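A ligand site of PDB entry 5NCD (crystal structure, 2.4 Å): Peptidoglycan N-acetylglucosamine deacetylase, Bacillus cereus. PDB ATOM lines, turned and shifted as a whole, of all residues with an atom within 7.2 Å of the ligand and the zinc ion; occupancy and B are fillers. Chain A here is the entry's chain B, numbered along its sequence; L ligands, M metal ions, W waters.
OD2 of Asp 50 is in hydrogen-bond range of N5 of the ligand (3.2 Å).
The backbone NH (N) of Tyr 141 lies close to an oxygen (O1) of the ligand (3.0 Å).
A ring nitrogen (NE2) of His 204 is in hydrogen-bond range of a nitrogen (N5) of the ligand, at 3.0 Å.
NH1 of Arg 138 lies within salt-bridge range of OD1 of Asp 50.
The backbone NH (N) of Asp 50 sits at hydrogen-bond distance from the backbone carbonyl oxygen (O) of Met 203 (3.1 Å).
ND1 of His 100 is in hydrogen-bond range of O of Arg 138, 2.4 Å away.
OH of Tyr 141 is in hydrogen-bond range of O of His 104.
The backbone NH (N) of His 104 sits at hydrogen-bond distance from the side-chain hydroxyl (OG) of Ser 101 (3.2 Å).
The backbone NH (N) of Asp 51 is in hydrogen-bond range of the backbone carbonyl oxygen (O) of Phe 74, 3.1 Å away.
Pro 140 touches the ligand.
Trp 165 touches the ligand (CH2 to N1, 3.8 Å).
Trp 172 touches the ligand (CZ2 to N3, 3.8 Å).
Leu 202 touches the ligand.
Hydrophobic or aromatic side chains that line the ligand: His 100, His 104, Tyr 141, Trp 165, Trp 172, Leu 202 and His 204.
Within 4 Å of the ligand: Asp 50, Asp 51, His 100, His 104, Pro 140, Tyr 141, Trp 165, Trp 172, Leu 202 and His 204.
The nearest printed residue that does not touch the ligand is Gly 142 (4.3 Å).
Of the 20 residues printed, 3 come within 4 Å of the zinc ion.
NE2 of His 104 is bound to the zinc ion (2.1 Å).
A ring nitrogen (NE2) of His 100 is bound to the zinc ion, 2.2 Å away.
The zinc ion is bound by O2 of the ligand (2.2 Å).
OD1 of Asp 51 binds the zinc ion, 2.2 Å away.
An oxygen (O1) of the ligand binds the zinc ion.
Water W1 is bound to the zinc ion (2.4 Å).
The zinc ion has six donor atoms within binding distance.
Water W1 lies within hydrogen-bond range of OD2 of Asp 51 (2.8 Å), NE2 of His 204 (3.3 Å) and N5 of the ligand (3.3 Å).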
ATOM      1  N   PHE A  49       6.448  24.793  26.558  1.00  0.00           N
ATOM      2  CA  PHE A  49       5.330  25.700  26.421  1.00  0.00           C
ATOM      3  C   PHE A  49       5.864  26.973  25.816  1.00  0.00           C
ATOM      4  O   PHE A  49       6.890  27.519  26.246  1.00  0.00           O
ATOM      5  CB  PHE A  49       4.672  25.931  27.786  1.00  0.00           C
ATOM      6  CG  PHE A  49       4.168  24.658  28.440  1.00  0.00           C
ATOM      7  CD1 PHE A  49       2.919  24.148  28.153  1.00  0.00           C
ATOM      8  CD2 PHE A  49       4.968  23.966  29.339  1.00  0.00           C
ATOM      9  CE1 PHE A  49       2.465  22.991  28.758  1.00  0.00           C
ATOM     10  CE2 PHE A  49       4.526  22.791  29.933  1.00  0.00           C
ATOM     11  CZ  PHE A  49       3.274  22.304  29.643  1.00  0.00           C
ATOM     12  N   ASP A  50       5.135  27.427  24.801  1.00  0.00           N
ATOM     13  CA  ASP A  50       5.576  28.493  23.930  1.00  0.00           C
ATOM     14  C   ASP A  50       4.680  29.720  23.992  1.00  0.00           C
ATOM     15  O   ASP A  50       3.485  29.629  24.319  1.00  0.00           O
ATOM     16  CB  ASP A  50       5.605  28.011  22.455  1.00  0.00           C
ATOM     17  CG  ASP A  50       6.712  26.985  22.156  1.00  0.00           C
ATOM     18  OD1 ASP A  50       7.240  26.307  23.078  1.00  0.00           O
ATOM     19  OD2 ASP A  50       7.060  26.857  20.958  1.00  0.00           O
ATOM     20  N   ASP A  51       5.278  30.854  23.624  1.00  0.00           N
ATOM     21  CA  ASP A  51       4.625  32.155  23.436  1.00  0.00           C
ATOM     22  C   ASP A  51       4.293  32.876  24.751  1.00  0.00           C
ATOM     23  O   ASP A  51       3.769  33.987  24.729  1.00  0.00           O
ATOM     24  CB  ASP A  51       3.339  32.027  22.600  1.00  0.00           C
ATOM     25  CG  ASP A  51       3.568  31.439  21.192  1.00  0.00           C
ATOM     26  OD1 ASP A  51       4.718  31.246  20.713  1.00  0.00           O
ATOM     27  OD2 ASP A  51       2.545  31.171  20.545  1.00  0.00           O
ATOM     28  N   PHE A  74       9.453  28.916  26.437  1.00  0.00           N
ATOM     29  CA  PHE A  74      10.052  29.676  25.369  1.00  0.00           C
ATOM     30  C   PHE A  74       9.237  30.901  25.269  1.00  0.00           C
ATOM     31  O   PHE A  74       8.048  30.820  24.933  1.00  0.00           O
ATOM     32  CB  PHE A  74      10.060  28.881  24.060  1.00  0.00           C
ATOM     33  CG  PHE A  74      10.934  27.677  24.090  1.00  0.00           C
ATOM     34  CD1 PHE A  74      12.327  27.821  24.110  1.00  0.00           C
ATOM     35  CD2 PHE A  74      10.388  26.401  24.087  1.00  0.00           C
ATOM     36  CE1 PHE A  74      13.162  26.700  24.108  1.00  0.00           C
ATOM     37  CE2 PHE A  74      11.224  25.277  24.099  1.00  0.00           C
ATOM     38  CZ  PHE A  74      12.616  25.430  24.113  1.00  0.00           C
ATOM     39  N   ILE A  76       8.055  34.990  24.508  1.00  0.00           N
ATOM     40  CA  ILE A  76       8.104  36.173  23.672  1.00  0.00           C
ATOM     41  C   ILE A  76       8.474  37.325  24.592  1.00  0.00           C
ATOM     42  O   ILE A  76       7.869  37.498  25.639  1.00  0.00           O
ATOM     43  CB  ILE A  76       6.750  36.452  22.974  1.00  0.00           C
ATOM     44  CG1 ILE A  76       6.294  35.258  22.148  1.00  0.00           C
ATOM     45  CG2 ILE A  76       6.834  37.681  22.074  1.00  0.00           C
ATOM     46  CD1 ILE A  76       4.992  35.512  21.386  1.00  0.00           C
ATOM     47  N   HIS A 100      11.940  32.738  22.593  1.00  0.00           N
ATOM     48  CA  HIS A 100      11.018  32.551  21.470  1.00  0.00           C
ATOM     49  C   HIS A 100      10.814  33.872  20.697  1.00  0.00           C
ATOM     50  O   HIS A 100       9.758  34.077  20.099  1.00  0.00           O
ATOM     51  CB  HIS A 100       9.687  31.984  21.967  1.00  0.00           C
ATOM     52  CG  HIS A 100       8.827  31.348  20.899  1.00  0.00           C
ATOM     53  ND1 HIS A 100       9.294  30.384  20.035  1.00  0.00           N
ATOM     54  CD2 HIS A 100       7.514  31.526  20.591  1.00  0.00           C
ATOM     55  CE1 HIS A 100       8.311  30.007  19.234  1.00  0.00           C
ATOM     56  NE2 HIS A 100       7.226  30.684  19.546  1.00  0.00           N
ATOM     57  N   SER A 101      11.830  34.723  20.715  1.00  0.00           N
ATOM     58  CA  SER A 101      11.911  36.003  19.984  1.00  0.00           C
ATOM     59  C   SER A 101      11.202  37.184  20.647  1.00  0.00           C
ATOM     60  O   SER A 101      10.575  37.062  21.705  1.00  0.00           O
ATOM     61  CB  SER A 101      11.395  35.877  18.546  1.00  0.00           C
ATOM     62  OG  SER A 101      10.003  35.616  18.531  1.00  0.00           O
ATOM     63  N   HIS A 104       7.894  37.517  17.013  1.00  0.00           N
ATOM     64  CA  HIS A 104       7.200  36.305  16.507  1.00  0.00           C
ATOM     65  C   HIS A 104       6.714  36.508  15.072  1.00  0.00           C
ATOM     66  O   HIS A 104       5.732  35.915  14.674  1.00  0.00           O
ATOM     67  CB  HIS A 104       6.013  35.922  17.394  1.00  0.00           C
ATOM     68  CG  HIS A 104       5.603  34.476  17.295  1.00  0.00           C
ATOM     69  ND1 HIS A 104       5.088  33.918  16.149  1.00  0.00           N
ATOM     70  CD2 HIS A 104       5.659  33.469  18.202  1.00  0.00           C
ATOM     71  CE1 HIS A 104       4.835  32.634  16.347  1.00  0.00           C
ATOM     72  NE2 HIS A 104       5.169  32.333  17.599  1.00  0.00           N
ATOM     73  N   ARG A 138      13.710  28.464  20.715  1.00  0.00           N
ATOM     74  CA  ARG A 138      12.670  27.731  19.999  1.00  0.00           C
ATOM     75  C   ARG A 138      12.117  28.683  18.969  1.00  0.00           C
ATOM     76  O   ARG A 138      11.522  29.708  19.321  1.00  0.00           O
ATOM     77  CB  ARG A 138      11.586  27.225  20.959  1.00  0.00           C
ATOM     78  CG  ARG A 138      10.184  27.044  20.390  1.00  0.00           C
ATOM     79  CD  ARG A 138      10.032  25.823  19.515  1.00  0.00           C
ATOM     80  NE  ARG A 138      10.383  24.533  20.132  1.00  0.00           N
ATOM     81  CZ  ARG A 138       9.729  23.939  21.114  1.00  0.00           C
ATOM     82  NH1 ARG A 138       8.674  24.510  21.663  1.00  0.00           N
ATOM     83  NH2 ARG A 138      10.131  22.754  21.571  1.00  0.00           N
ATOM     84  N   PRO A 139      12.363  28.352  17.694  1.00  0.00           N
ATOM     85  CA  PRO A 139      11.999  29.211  16.567  1.00  0.00           C
ATOM     86  C   PRO A 139      10.494  29.297  16.440  1.00  0.00           C
ATOM     87  O   PRO A 139       9.836  28.269  16.557  1.00  0.00           O
ATOM     88  CB  PRO A 139      12.591  28.501  15.342  1.00  0.00           C
ATOM     89  CG  PRO A 139      13.344  27.325  15.873  1.00  0.00           C
ATOM     90  CD  PRO A 139      12.854  27.034  17.239  1.00  0.00           C
ATOM     91  N   PRO A 140       9.960  30.506  16.222  1.00  0.00           N
ATOM     92  CA  PRO A 140       8.539  30.658  15.890  1.00  0.00           C
ATOM     93  C   PRO A 140       8.233  29.993  14.550  1.00  0.00           C
ATOM     94  O   PRO A 140       9.056  30.078  13.645  1.00  0.00           O
ATOM     95  CB  PRO A 140       8.359  32.183  15.809  1.00  0.00           C
ATOM     96  CG  PRO A 140       9.485  32.745  16.617  1.00  0.00           C
ATOM     97  CD  PRO A 140      10.634  31.812  16.380  1.00  0.00           C
ATOM     98  N   TYR A 141       7.068  29.341  14.454  1.00  0.00           N
ATOM     99  CA  TYR A 141       6.618  28.608  13.270  1.00  0.00           C
ATOM    100  C   TYR A 141       7.567  27.443  12.909  1.00  0.00           C
ATOM    101  O   TYR A 141       7.513  26.891  11.797  1.00  0.00           O
ATOM    102  CB  TYR A 141       6.446  29.558  12.072  1.00  0.00           C
ATOM    103  CG  TYR A 141       5.620  30.802  12.388  1.00  0.00           C
ATOM    104  CD1 TYR A 141       4.221  30.739  12.530  1.00  0.00           C
ATOM    105  CD2 TYR A 141       6.230  32.037  12.540  1.00  0.00           C
ATOM    106  CE1 TYR A 141       3.464  31.886  12.818  1.00  0.00           C
ATOM    107  CE2 TYR A 141       5.494  33.178  12.833  1.00  0.00           C
ATOM    108  CZ  TYR A 141       4.115  33.109  12.980  1.00  0.00           C
ATOM    109  OH  TYR A 141       3.417  34.272  13.284  1.00  0.00           O
ATOM    110  N   GLY A 142       8.409  27.070  13.866  1.00  0.00           N
ATOM    111  CA  GLY A 142       9.426  26.043  13.670  1.00  0.00           C
ATOM    112  C   GLY A 142      10.601  26.550  12.846  1.00  0.00           C
ATOM    113  O   GLY A 142      10.494  27.578  12.161  1.00  0.00           O
ATOM    114  N   TRP A 165      10.520  20.321  17.813  1.00  0.00           N
ATOM    115  CA  TRP A 165       9.746  19.378  18.608  1.00  0.00           C
ATOM    116  C   TRP A 165       9.552  18.070  17.846  1.00  0.00           C
ATOM    117  O   TRP A 165       9.650  18.040  16.631  1.00  0.00           O
ATOM    118  CB  TRP A 165       8.378  19.962  18.965  1.00  0.00           C
ATOM    119  CG  TRP A 165       7.606  20.333  17.774  1.00  0.00           C
ATOM    120  CD1 TRP A 165       6.720  19.563  17.091  1.00  0.00           C
ATOM    121  CD2 TRP A 165       7.669  21.588  17.083  1.00  0.00           C
ATOM    122  NE1 TRP A 165       6.200  20.265  16.022  1.00  0.00           N
ATOM    123  CE2 TRP A 165       6.769  21.501  15.979  1.00  0.00           C
ATOM    124  CE3 TRP A 165       8.364  22.783  17.289  1.00  0.00           C
ATOM    125  CZ2 TRP A 165       6.558  22.561  15.101  1.00  0.00           C
ATOM    126  CZ3 TRP A 165       8.185  23.821  16.391  1.00  0.00           C
ATOM    127  CH2 TRP A 165       7.288  23.701  15.309  1.00  0.00           C
ATOM    128  N   ASP A 168       3.623  17.468  18.074  1.00  0.00           N
ATOM    129  CA  ASP A 168       2.836  18.701  17.983  1.00  0.00           C
ATOM    130  C   ASP A 168       1.434  18.466  18.523  1.00  0.00           C
ATOM    131  O   ASP A 168       0.608  17.815  17.885  1.00  0.00           O
ATOM    132  CB  ASP A 168       2.774  19.212  16.538  1.00  0.00           C
ATOM    133  CG  ASP A 168       2.032  20.505  16.422  1.00  0.00           C
ATOM    134  OD1 ASP A 168       1.416  20.911  17.425  1.00  0.00           O
ATOM    135  OD2 ASP A 168       2.071  21.125  15.330  1.00  0.00           O
ATOM    136  N   TRP A 172      -3.382  24.831  20.116  1.00  0.00           N
ATOM    137  CA  TRP A 172      -3.975  26.141  19.878  1.00  0.00           C
ATOM    138  C   TRP A 172      -5.071  26.119  18.829  1.00  0.00           C
ATOM    139  O   TRP A 172      -5.766  27.118  18.643  1.00  0.00           O
ATOM    140  CB  TRP A 172      -2.912  27.123  19.431  1.00  0.00           C
ATOM    141  CG  TRP A 172      -2.204  26.692  18.211  1.00  0.00           C
ATOM    142  CD1 TRP A 172      -1.072  25.953  18.145  1.00  0.00           C
ATOM    143  CD2 TRP A 172      -2.586  26.967  16.854  1.00  0.00           C
ATOM    144  NE1 TRP A 172      -0.716  25.738  16.848  1.00  0.00           N
ATOM    145  CE2 TRP A 172      -1.629  26.351  16.030  1.00  0.00           C
ATOM    146  CE3 TRP A 172      -3.637  27.665  16.259  1.00  0.00           C
ATOM    147  CZ2 TRP A 172      -1.681  26.417  14.636  1.00  0.00           C
ATOM    148  CZ3 TRP A 172      -3.688  27.723  14.870  1.00  0.00           C
ATOM    149  CH2 TRP A 172      -2.710  27.103  14.074  1.00  0.00           C
ATOM    150  N   ARG A 173      -5.204  25.017  18.116  1.00  0.00           N
ATOM    151  CA  ARG A 173      -6.243  24.916  17.086  1.00  0.00           C
ATOM    152  C   ARG A 173      -7.611  24.636  17.716  1.00  0.00           C
ATOM    153  O   ARG A 173      -8.609  25.098  17.230  1.00  0.00           O
ATOM    154  CB  ARG A 173      -5.877  23.835  16.077  1.00  0.00           C
ATOM    155  CG  ARG A 173      -4.603  24.150  15.347  1.00  0.00           C
ATOM    156  CD  ARG A 173      -4.182  23.020  14.421  1.00  0.00           C
ATOM    157  NE  ARG A 173      -3.268  23.522  13.406  1.00  0.00           N
ATOM    158  CZ  ARG A 173      -3.639  23.905  12.195  1.00  0.00           C
ATOM    159  NH1 ARG A 173      -4.920  23.842  11.842  1.00  0.00           N
ATOM    160  NH2 ARG A 173      -2.741  24.365  11.338  1.00  0.00           N
ATOM    161  N   LEU A 202       5.224  19.885  21.942  1.00  0.00           N
ATOM    162  CA  LEU A 202       4.983  21.294  21.694  1.00  0.00           C
ATOM    163  C   LEU A 202       3.611  21.709  22.196  1.00  0.00           C
ATOM    164  O   LEU A 202       2.604  21.178  21.732  1.00  0.00           O
ATOM    165  CB  LEU A 202       5.111  21.589  20.221  1.00  0.00           C
ATOM    166  CG  LEU A 202       4.582  22.952  19.761  1.00  0.00           C
ATOM    167  CD1 LEU A 202       5.323  24.094  20.410  1.00  0.00           C
ATOM    168  CD2 LEU A 202       4.703  22.997  18.235  1.00  0.00           C
ATOM    169  N   MET A 203       3.570  22.636  23.144  1.00  0.00           N
ATOM    170  CA  MET A 203       2.311  23.237  23.567  1.00  0.00           C
ATOM    171  C   MET A 203       2.476  24.735  23.690  1.00  0.00           C
ATOM    172  O   MET A 203       3.518  25.289  23.341  1.00  0.00           O
ATOM    173  CB  MET A 203       1.819  22.643  24.891  1.00  0.00           C
ATOM    174  CG  MET A 203       1.346  21.222  24.748  1.00  0.00           C
ATOM    175  SD  MET A 203       0.947  20.386  26.295  1.00  0.00           S
ATOM    176  CE  MET A 203      -0.740  20.945  26.495  1.00  0.00           C
ATOM    177  N   HIS A 204       1.415  25.374  24.159  1.00  0.00           N
ATOM    178  CA  HIS A 204       1.372  26.828  24.300  1.00  0.00           C
ATOM    179  C   HIS A 204       0.676  27.140  25.610  1.00  0.00           C
ATOM    180  O   HIS A 204      -0.473  26.756  25.795  1.00  0.00           O
ATOM    181  CB  HIS A 204       0.626  27.466  23.128  1.00  0.00           C
ATOM    182  CG  HIS A 204       1.308  27.309  21.800  1.00  0.00           C
ATOM    183  ND1 HIS A 204       1.447  26.092  21.166  1.00  0.00           N
ATOM    184  CD2 HIS A 204       1.873  28.231  20.984  1.00  0.00           C
ATOM    185  CE1 HIS A 204       2.079  26.268  20.024  1.00  0.00           C
ATOM    186  NE2 HIS A 204       2.332  27.563  19.879  1.00  0.00           N
HETATM  187  N1  LIG L   1       4.458  25.602  16.902  1.00  0.00           N
HETATM  188  C1  LIG L   1       4.830  26.880  16.237  1.00  0.00           C
HETATM  189  C2  LIG L   1       3.693  27.312  15.321  1.00  0.00           C
HETATM  190  C3  LIG L   1       3.481  26.288  14.207  1.00  0.00           C
HETATM  191  C4  LIG L   1       2.268  26.662  13.360  1.00  0.00           C
HETATM  192  N2  LIG L   1       2.258  28.074  13.064  1.00  0.00           N
HETATM  193  C5  LIG L   1       1.391  28.902  13.648  1.00  0.00           C
HETATM  194  N3  LIG L   1       1.211  28.838  14.897  1.00  0.00           N
HETATM  195  N4  LIG L   1       0.669  29.841  12.879  1.00  0.00           N
HETATM  196  C6  LIG L   1       5.108  27.947  17.242  1.00  0.00           C
HETATM  197  O1  LIG L   1       5.392  29.105  16.901  1.00  0.00           O
HETATM  198  N5  LIG L   1       5.054  27.600  18.515  1.00  0.00           N
HETATM  199  O2  LIG L   1       5.331  28.567  19.478  1.00  0.00           O
HETATM  200 ZN    ZN M   1       5.243  30.587  18.676  1.00  0.00          ZN
HETATM  201  O   HOH W   1       3.032  30.133  17.988  1.00  0.00           O
